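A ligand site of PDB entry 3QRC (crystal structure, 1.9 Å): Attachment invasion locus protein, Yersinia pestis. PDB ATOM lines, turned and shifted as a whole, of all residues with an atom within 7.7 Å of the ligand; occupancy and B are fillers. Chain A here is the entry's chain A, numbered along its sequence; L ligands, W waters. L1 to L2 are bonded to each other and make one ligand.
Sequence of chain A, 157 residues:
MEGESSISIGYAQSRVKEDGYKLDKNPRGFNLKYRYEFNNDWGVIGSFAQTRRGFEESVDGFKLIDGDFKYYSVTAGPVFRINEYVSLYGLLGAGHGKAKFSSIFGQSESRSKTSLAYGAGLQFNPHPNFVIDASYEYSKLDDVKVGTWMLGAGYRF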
ATOM      1  N   GLN A  50     -23.305  13.116  10.833  1.00  0.00           N
ATOM      2  CA  GLN A  50     -23.138  14.530  11.166  1.00  0.00           C
ATOM      3  C   GLN A  50     -23.595  15.393  10.006  1.00  0.00           C
ATOM      4  O   GLN A  50     -23.259  15.131   8.851  1.00  0.00           O
ATOM      5  CB  GLN A  50     -21.681  14.835  11.480  1.00  0.00           C
ATOM      6  CG  GLN A  50     -21.395  16.298  11.727  1.00  0.00           C
ATOM      7  CD  GLN A  50     -19.925  16.538  12.030  1.00  0.00           C
ATOM      8  OE1 GLN A  50     -19.467  16.248  13.134  1.00  0.00           O
ATOM      9  NE2 GLN A  50     -19.188  17.058  11.062  1.00  0.00           N
ATOM     10  N   ARG A  52     -24.232  19.742   8.969  1.00  0.00           N
ATOM     11  CA  ARG A  52     -23.896  21.088   9.378  1.00  0.00           C
ATOM     12  C   ARG A  52     -24.446  22.090   8.404  1.00  0.00           C
ATOM     13  O   ARG A  52     -24.586  21.820   7.220  1.00  0.00           O
ATOM     14  CB  ARG A  52     -22.388  21.283   9.386  1.00  0.00           C
ATOM     15  CG  ARG A  52     -21.634  20.523  10.446  1.00  0.00           C
ATOM     16  CD  ARG A  52     -20.154  20.912  10.412  1.00  0.00           C
ATOM     17  NE  ARG A  52     -19.447  20.422  11.591  1.00  0.00           N
ATOM     18  CZ  ARG A  52     -18.151  20.638  11.830  1.00  0.00           C
ATOM     19  NH1 ARG A  52     -17.422  21.316  10.958  1.00  0.00           N
ATOM     20  NH2 ARG A  52     -17.598  20.156  12.940  1.00  0.00           N
ATOM     21  N   ASP A  68     -23.165  28.612  13.172  1.00  0.00           N
ATOM     22  CA  ASP A  68     -23.360  27.369  12.480  1.00  0.00           C
ATOM     23  C   ASP A  68     -24.196  26.455  13.319  1.00  0.00           C
ATOM     24  O   ASP A  68     -24.232  26.555  14.547  1.00  0.00           O
ATOM     25  CB  ASP A  68     -22.023  26.709  12.096  1.00  0.00           C
ATOM     26  CG  ASP A  68     -21.220  26.288  13.306  1.00  0.00           C
ATOM     27  OD1 ASP A  68     -21.204  25.081  13.597  1.00  0.00           O
ATOM     28  OD2 ASP A  68     -20.612  27.173  13.933  1.00  0.00           O
ATOM     29  N   PHE A  69     -24.878  25.564  12.633  1.00  0.00           N
ATOM     30  CA  PHE A  69     -25.747  24.607  13.234  1.00  0.00           C
ATOM     31  C   PHE A  69     -25.082  23.281  12.936  1.00  0.00           C
ATOM     32  O   PHE A  69     -24.583  23.081  11.833  1.00  0.00           O
ATOM     33  CB  PHE A  69     -27.112  24.729  12.562  1.00  0.00           C
ATOM     34  CG  PHE A  69     -27.701  26.101  12.709  1.00  0.00           C
ATOM     35  CD1 PHE A  69     -28.499  26.413  13.811  1.00  0.00           C
ATOM     36  CD2 PHE A  69     -27.434  27.092  11.776  1.00  0.00           C
ATOM     37  CE1 PHE A  69     -29.022  27.681  13.960  1.00  0.00           C
ATOM     38  CE2 PHE A  69     -27.976  28.371  11.914  1.00  0.00           C
ATOM     39  CZ  PHE A  69     -28.772  28.671  13.010  1.00  0.00           C
ATOM     40  N   LYS A  70     -25.008  22.415  13.948  1.00  0.00           N
ATOM     41  CA  LYS A  70     -24.423  21.094  13.784  1.00  0.00           C
ATOM     42  C   LYS A  70     -25.276  20.058  14.497  1.00  0.00           C
ATOM     43  O   LYS A  70     -25.705  20.280  15.632  1.00  0.00           O
ATOM     44  CB  LYS A  70     -23.018  21.052  14.376  1.00  0.00           C
ATOM     45  CG  LYS A  70     -22.377  19.664  14.289  1.00  0.00           C
ATOM     46  CD  LYS A  70     -20.927  19.657  14.793  1.00  0.00           C
ATOM     47  CE  LYS A  70     -20.861  19.713  16.319  1.00  0.00           C
ATOM     48  NZ  LYS A  70     -19.480  19.464  16.827  1.00  0.00           N
ATOM     49  N   TYR A  71     -25.489  18.920  13.847  1.00  0.00           N
ATOM     50  CA  TYR A  71     -26.142  17.784  14.489  1.00  0.00           C
ATOM     51  C   TYR A  71     -25.237  16.594  14.287  1.00  0.00           C
ATOM     52  O   TYR A  71     -24.727  16.380  13.198  1.00  0.00           O
ATOM     53  CB  TYR A  71     -27.468  17.516  13.787  1.00  0.00           C
ATOM     54  CG  TYR A  71     -28.135  16.230  14.184  1.00  0.00           C
ATOM     55  CD1 TYR A  71     -28.875  16.122  15.372  1.00  0.00           C
ATOM     56  CD2 TYR A  71     -28.045  15.101  13.370  1.00  0.00           C
ATOM     57  CE1 TYR A  71     -29.490  14.921  15.727  1.00  0.00           C
ATOM     58  CE2 TYR A  71     -28.651  13.904  13.722  1.00  0.00           C
ATOM     59  CZ  TYR A  71     -29.380  13.829  14.885  1.00  0.00           C
ATOM     60  OH  TYR A  71     -29.994  12.618  15.199  1.00  0.00           O
ATOM     61  N   TYR A  72     -25.021  15.797  15.332  1.00  0.00           N
ATOM     62  CA  TYR A  72     -24.401  14.489  15.058  1.00  0.00           C
ATOM     63  C   TYR A  72     -25.043  13.440  15.927  1.00  0.00           C
ATOM     64  O   TYR A  72     -25.647  13.760  16.944  1.00  0.00           O
ATOM     65  CB  TYR A  72     -22.887  14.528  15.251  1.00  0.00           C
ATOM     66  CG  TYR A  72     -22.435  14.863  16.651  1.00  0.00           C
ATOM     67  CD1 TYR A  72     -22.211  16.178  17.029  1.00  0.00           C
ATOM     68  CD2 TYR A  72     -22.244  13.856  17.603  1.00  0.00           C
ATOM     69  CE1 TYR A  72     -21.800  16.487  18.316  1.00  0.00           C
ATOM     70  CE2 TYR A  72     -21.843  14.158  18.884  1.00  0.00           C
ATOM     71  CZ  TYR A  72     -21.619  15.479  19.238  1.00  0.00           C
ATOM     72  OH  TYR A  72     -21.208  15.788  20.526  1.00  0.00           O
ATOM     73  N   HIS A  96     -27.075  14.843  19.165  1.00  0.00           N
ATOM     74  CA  HIS A  96     -26.671  16.087  19.803  1.00  0.00           C
ATOM     75  C   HIS A  96     -26.818  17.202  18.781  1.00  0.00           C
ATOM     76  O   HIS A  96     -26.261  17.133  17.673  1.00  0.00           O
ATOM     77  CB  HIS A  96     -25.217  16.001  20.259  1.00  0.00           C
ATOM     78  CG  HIS A  96     -24.726  17.249  20.920  1.00  0.00           C
ATOM     79  ND1 HIS A  96     -24.979  17.539  22.243  1.00  0.00           N
ATOM     80  CD2 HIS A  96     -24.008  18.287  20.440  1.00  0.00           C
ATOM     81  CE1 HIS A  96     -24.413  18.690  22.556  1.00  0.00           C
ATOM     82  NE2 HIS A  96     -23.825  19.175  21.479  1.00  0.00           N
ATOM     83  N   GLY A  97     -27.564  18.241  19.156  1.00  0.00           N
ATOM     84  CA  GLY A  97     -27.744  19.401  18.287  1.00  0.00           C
ATOM     85  C   GLY A  97     -27.148  20.645  18.950  1.00  0.00           C
ATOM     86  O   GLY A  97     -27.181  20.793  20.181  1.00  0.00           O
ATOM     87  N   LYS A  98     -26.587  21.513  18.120  1.00  0.00           N
ATOM     88  CA  LYS A  98     -25.833  22.673  18.585  1.00  0.00           C
ATOM     89  C   LYS A  98     -26.029  23.808  17.609  1.00  0.00           C
ATOM     90  O   LYS A  98     -25.965  23.620  16.386  1.00  0.00           O
ATOM     91  CB  LYS A  98     -24.338  22.302  18.659  1.00  0.00           C
ATOM     92  CG  LYS A  98     -23.375  23.466  18.950  1.00  0.00           C
ATOM     93  CD  LYS A  98     -23.170  23.653  20.443  1.00  0.00           C
ATOM     94  CE  LYS A  98     -21.872  24.396  20.762  1.00  0.00           C
ATOM     95  NZ  LYS A  98     -20.705  23.476  20.777  1.00  0.00           N
ATOM     96  N   ALA A  99     -26.296  25.003  18.132  1.00  0.00           N
ATOM     97  CA  ALA A  99     -26.340  26.190  17.323  1.00  0.00           C
ATOM     98  C   ALA A  99     -25.392  27.187  17.980  1.00  0.00           C
ATOM     99  O   ALA A  99     -25.532  27.477  19.172  1.00  0.00           O
ATOM    100  CB  ALA A  99     -27.746  26.765  17.287  1.00  0.00           C
ATOM    101  N   LYS A 100     -24.421  27.668  17.205  1.00  0.00           N
ATOM    102  CA  LYS A 100     -23.341  28.494  17.745  1.00  0.00           C
ATOM    103  C   LYS A 100     -23.342  29.816  17.020  1.00  0.00           C
ATOM    104  O   LYS A 100     -23.502  29.858  15.792  1.00  0.00           O
ATOM    105  CB  LYS A 100     -22.005  27.777  17.544  1.00  0.00           C
ATOM    106  CG  LYS A 100     -20.781  28.530  18.049  1.00  0.00           C
ATOM    107  CD  LYS A 100     -19.692  27.536  18.431  1.00  0.00           C
ATOM    108  CE  LYS A 100     -18.305  28.134  18.319  1.00  0.00           C
ATOM    109  N   SER A 108     -20.053  35.425  21.865  1.00  0.00           N
ATOM    110  CA  SER A 108     -19.785  34.062  21.402  1.00  0.00           C
ATOM    111  C   SER A 108     -20.552  33.047  22.252  1.00  0.00           C
ATOM    112  O   SER A 108     -20.137  32.760  23.363  1.00  0.00           O
ATOM    113  CB  SER A 108     -18.286  33.757  21.408  1.00  0.00           C
ATOM    114  OG  SER A 108     -18.023  32.541  20.720  1.00  0.00           O
ATOM    115  N   GLU A 109     -21.670  32.533  21.748  1.00  0.00           N
ATOM    116  CA  GLU A 109     -22.572  31.762  22.602  1.00  0.00           C
ATOM    117  C   GLU A 109     -23.238  30.655  21.807  1.00  0.00           C
ATOM    118  O   GLU A 109     -23.353  30.771  20.598  1.00  0.00           O
ATOM    119  CB  GLU A 109     -23.651  32.664  23.193  1.00  0.00           C
ATOM    120  CG  GLU A 109     -24.426  33.465  22.154  1.00  0.00           C
ATOM    121  N   SER A 110     -23.699  29.617  22.494  1.00  0.00           N
ATOM    122  CA  SER A 110     -24.322  28.504  21.811  1.00  0.00           C
ATOM    123  C   SER A 110     -25.524  27.953  22.594  1.00  0.00           C
ATOM    124  O   SER A 110     -25.648  28.163  23.800  1.00  0.00           O
ATOM    125  CB  SER A 110     -23.290  27.398  21.553  1.00  0.00           C
ATOM    126  OG  SER A 110     -22.614  27.024  22.750  1.00  0.00           O
ATOM    127  N   ARG A 111     -26.407  27.275  21.884  1.00  0.00           N
ATOM    128  CA  ARG A 111     -27.430  26.461  22.540  1.00  0.00           C
ATOM    129  C   ARG A 111     -27.300  25.020  22.048  1.00  0.00           C
ATOM    130  O   ARG A 111     -27.067  24.792  20.869  1.00  0.00           O
ATOM    131  CB  ARG A 111     -28.820  26.987  22.237  1.00  0.00           C
ATOM    132  CG  ARG A 111     -29.874  26.264  23.041  1.00  0.00           C
ATOM    133  CD  ARG A 111     -31.100  27.116  23.322  1.00  0.00           C
ATOM    134  NE  ARG A 111     -32.189  26.263  23.779  1.00  0.00           N
ATOM    135  CZ  ARG A 111     -32.397  25.926  25.038  1.00  0.00           C
ATOM    136  NH1 ARG A 111     -31.579  26.367  25.988  1.00  0.00           N
ATOM    137  NH2 ARG A 111     -33.416  25.143  25.358  1.00  0.00           N
ATOM    138  N   SER A 112     -27.464  24.048  22.942  1.00  0.00           N
ATOM    139  CA  SER A 112     -27.243  22.647  22.557  1.00  0.00           C
ATOM    140  C   SER A 112     -28.142  21.736  23.353  1.00  0.00           C
ATOM    141  O   SER A 112     -28.643  22.120  24.412  1.00  0.00           O
ATOM    142  CB  SER A 112     -25.789  22.258  22.819  1.00  0.00           C
ATOM    143  OG  SER A 112     -25.524  22.242  24.211  1.00  0.00           O
ATOM    144  N   LYS A 113     -28.316  20.510  22.868  1.00  0.00           N
ATOM    145  CA  LYS A 113     -29.150  19.548  23.560  1.00  0.00           C
ATOM    146  C   LYS A 113     -28.757  18.177  23.086  1.00  0.00           C
ATOM    147  O   LYS A 113     -28.459  17.981  21.904  1.00  0.00           O
ATOM    148  CB  LYS A 113     -30.628  19.807  23.241  1.00  0.00           C
ATOM    149  CG  LYS A 113     -31.598  18.756  23.767  1.00  0.00           C
ATOM    150  CD  LYS A 113     -31.749  18.840  25.295  1.00  0.00           C
ATOM    151  CE  LYS A 113     -32.723  17.782  25.802  1.00  0.00           C
ATOM    152  NZ  LYS A 113     -32.938  17.923  27.280  1.00  0.00           N
ATOM    153  N   THR A 114     -28.739  17.223  24.000  1.00  0.00           N
ATOM    154  CA  THR A 114     -28.560  15.821  23.657  1.00  0.00           C
ATOM    155  C   THR A 114     -29.840  15.069  23.987  1.00  0.00           C
ATOM    156  O   THR A 114     -30.391  15.238  25.069  1.00  0.00           O
ATOM    157  CB  THR A 114     -27.428  15.202  24.470  1.00  0.00           C
ATOM    158  OG1 THR A 114     -26.202  15.884  24.198  1.00  0.00           O
ATOM    159  CG2 THR A 114     -27.282  13.716  24.131  1.00  0.00           C
HETATM  160  C1  LIG L   1     -17.348  20.859  22.219  1.00  0.00           C
HETATM  161  O1  LIG L   1     -16.722  20.523  23.034  1.00  0.00           O
HETATM  162  C2  LIG L   1     -17.106  21.233  24.417  1.00  0.00           C
HETATM  163  C3  LIG L   1     -16.054  20.948  25.526  1.00  0.00           C
HETATM  164  O2  LIG L   1     -16.265  19.722  26.153  1.00  0.00           O
HETATM  165  S1  LIG L   1     -15.119  18.853  26.999  1.00  0.00           S
HETATM  166  O3  LIG L   1     -13.951  19.143  26.296  1.00  0.00           O
HETATM  167  O4  LIG L   1     -15.406  17.282  27.008  1.00  0.00           O
HETATM  168  O5  LIG L   1     -14.885  19.636  28.379  1.00  0.00           O
HETATM  169  C4  LIG L   1     -18.630  21.005  24.901  1.00  0.00           C
HETATM  170  O6  LIG L   1     -18.791  21.932  25.920  1.00  0.00           O
HETATM  171  S2  LIG L   1     -19.164  21.553  27.434  1.00  0.00           S
HETATM  172  O7  LIG L   1     -17.863  21.005  28.100  1.00  0.00           O
HETATM  173  O8  LIG L   1     -20.253  20.443  27.334  1.00  0.00           O
HETATM  174  O9  LIG L   1     -19.638  22.767  28.264  1.00  0.00           O
HETATM  175  C5  LIG L   1     -19.360  21.085  24.102  1.00  0.00           C
HETATM  176  O10 LIG L   1     -20.630  20.690  24.366  1.00  0.00           O
HETATM  177  S3  LIG L   1     -21.907  21.586  23.982  1.00  0.00           S
HETATM  178  O11 LIG L   1     -22.160  21.375  22.486  1.00  0.00           O
HETATM  179  O12 LIG L   1     -23.110  20.979  24.633  1.00  0.00           O
HETATM  180  O13 LIG L   1     -21.705  23.089  24.232  1.00  0.00           O
HETATM  181  C6  LIG L   1     -18.864  20.386  22.628  1.00  0.00           C
HETATM  182  O14 LIG L   1     -19.703  20.704  21.581  1.00  0.00           O
HETATM  183  S4  LIG L   1     -20.114  19.561  20.498  1.00  0.00           S
HETATM  184  O15 LIG L   1     -18.869  19.153  19.705  1.00  0.00           O
HETATM  185  O16 LIG L   1     -21.075  20.191  19.473  1.00  0.00           O
HETATM  186  O17 LIG L   1     -20.762  18.437  21.265  1.00  0.00           O
HETATM  187  C1  LG2 L   2     -16.935  22.146  19.677  1.00  0.00           C
HETATM  188  C2  LG2 L   2     -16.399  22.530  20.922  1.00  0.00           C
HETATM  189  C3  LG2 L   2     -16.108  23.963  21.081  1.00  0.00           C
HETATM  190  C4  LG2 L   2     -14.635  23.957  20.822  1.00  0.00           C
HETATM  191  C5  LG2 L   2     -14.223  22.786  21.593  1.00  0.00           C
HETATM  192  C6  LG2 L   2     -14.050  22.944  23.125  1.00  0.00           C
HETATM  193  O1  LG2 L   2     -18.177  22.653  19.317  1.00  0.00           O
HETATM  194  O2  LG2 L   2     -19.898  23.851  17.887  1.00  0.00           O
HETATM  195  O3  LG2 L   2     -17.616  26.062  24.014  1.00  0.00           O
HETATM  196  O4  LG2 L   2     -15.112  26.362  18.981  1.00  0.00           O
HETATM  197  O5  LG2 L   2     -12.025  25.361  25.614  1.00  0.00           O
HETATM  198  O6  LG2 L   2     -17.358  22.251  21.968  1.00  0.00           O
HETATM  199  O7  LG2 L   2     -18.223  22.406  16.730  1.00  0.00           O
HETATM  200  O8  LG2 L   2     -18.876  24.761  22.383  1.00  0.00           O
HETATM  201  O9  LG2 L   2     -13.702  25.095  17.197  1.00  0.00           O
HETATM  202  O10 LG2 L   2     -13.623  23.334  26.275  1.00  0.00           O
HETATM  203  O11 LG2 L   2     -16.417  24.437  22.338  1.00  0.00           O
HETATM  204  O12 LG2 L   2     -17.599  24.749  17.673  1.00  0.00           O
HETATM  205  O13 LG2 L   2     -17.548  26.605  21.454  1.00  0.00           O
HETATM  206  O14 LG2 L   2     -12.726  25.848  19.594  1.00  0.00           O
HETATM  207  O15 LG2 L   2     -14.656  25.459  25.169  1.00  0.00           O
HETATM  208  O16 LG2 L   2     -14.338  23.888  19.465  1.00  0.00           O
HETATM  209  O17 LG2 L   2     -15.225  21.870  21.134  1.00  0.00           O
HETATM  210  O18 LG2 L   2     -13.039  23.754  23.739  1.00  0.00           O
HETATM  211  S1  LG2 L   2     -18.460  23.444  17.888  1.00  0.00           S
HETATM  212  S2  LG2 L   2     -17.572  25.505  22.560  1.00  0.00           S
HETATM  213  S3  LG2 L   2     -13.960  25.306  18.766  1.00  0.00           S
HETATM  214  S4  LG2 L   2     -13.339  24.530  25.211  1.00  0.00           S
HETATM  215  O   HOH W   1     -23.810  24.870  24.002  1.00  0.00           O
HETATM  216  O   HOH W   2     -22.125  24.268  15.944  1.00  0.00           O
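NZ of Lys 98 is in salt-bridge range of O8 of LG2 L2 (2.8 Å). An oxygen (O12) of LIG L1 lies within hydrogen-bond range of the side-chain hydroxyl (OG) of Ser 112 (2.8 Å). OH of Tyr 72 sits at hydrogen-bond distance from O17 of LIG L1 (2.8 Å). A ring nitrogen (NE2) of His 96 is in hydrogen-bond range of an oxygen (O11) of LIG L1 (2.9 Å). NZ of Lys 70 lies within salt-bridge range of O15 of LIG L1 (3.0 Å).
The backbone carbonyl oxygen (O) of Lys 98 lies within hydrogen-bond range of the backbone NH (N) of Lys 70, at 2.9 Å. The backbone carbonyl oxygen of Tyr 72 is in hydrogen-bond range of the backbone NH of His 96. ND1 of His 96 is in hydrogen-bond range of OG1 of Thr 114 (2.8 Å). The backbone NH (N) of Lys 100 sits at hydrogen-bond distance from the backbone carbonyl oxygen (O) of Asp 68, 2.9 Å away.
Merely in contact with the ligand: Lys 100 (3.5 Å). Hydrophobic or aromatic side chains that line the ligand: Tyr 72 and His 96. The nearest printed residue that does not touch the ligand is Ser 110 (4.3 Å).
Water W1 lies within hydrogen-bond range of the side-chain hydroxyl of Ser 110, an oxygen (O13) of LIG L1 and the side-chain hydroxyl of Ser 112. Water W2 bridges OD1 of Asp 68 (2.6 Å) and O2 of LG2 L2 (3.0 Å).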
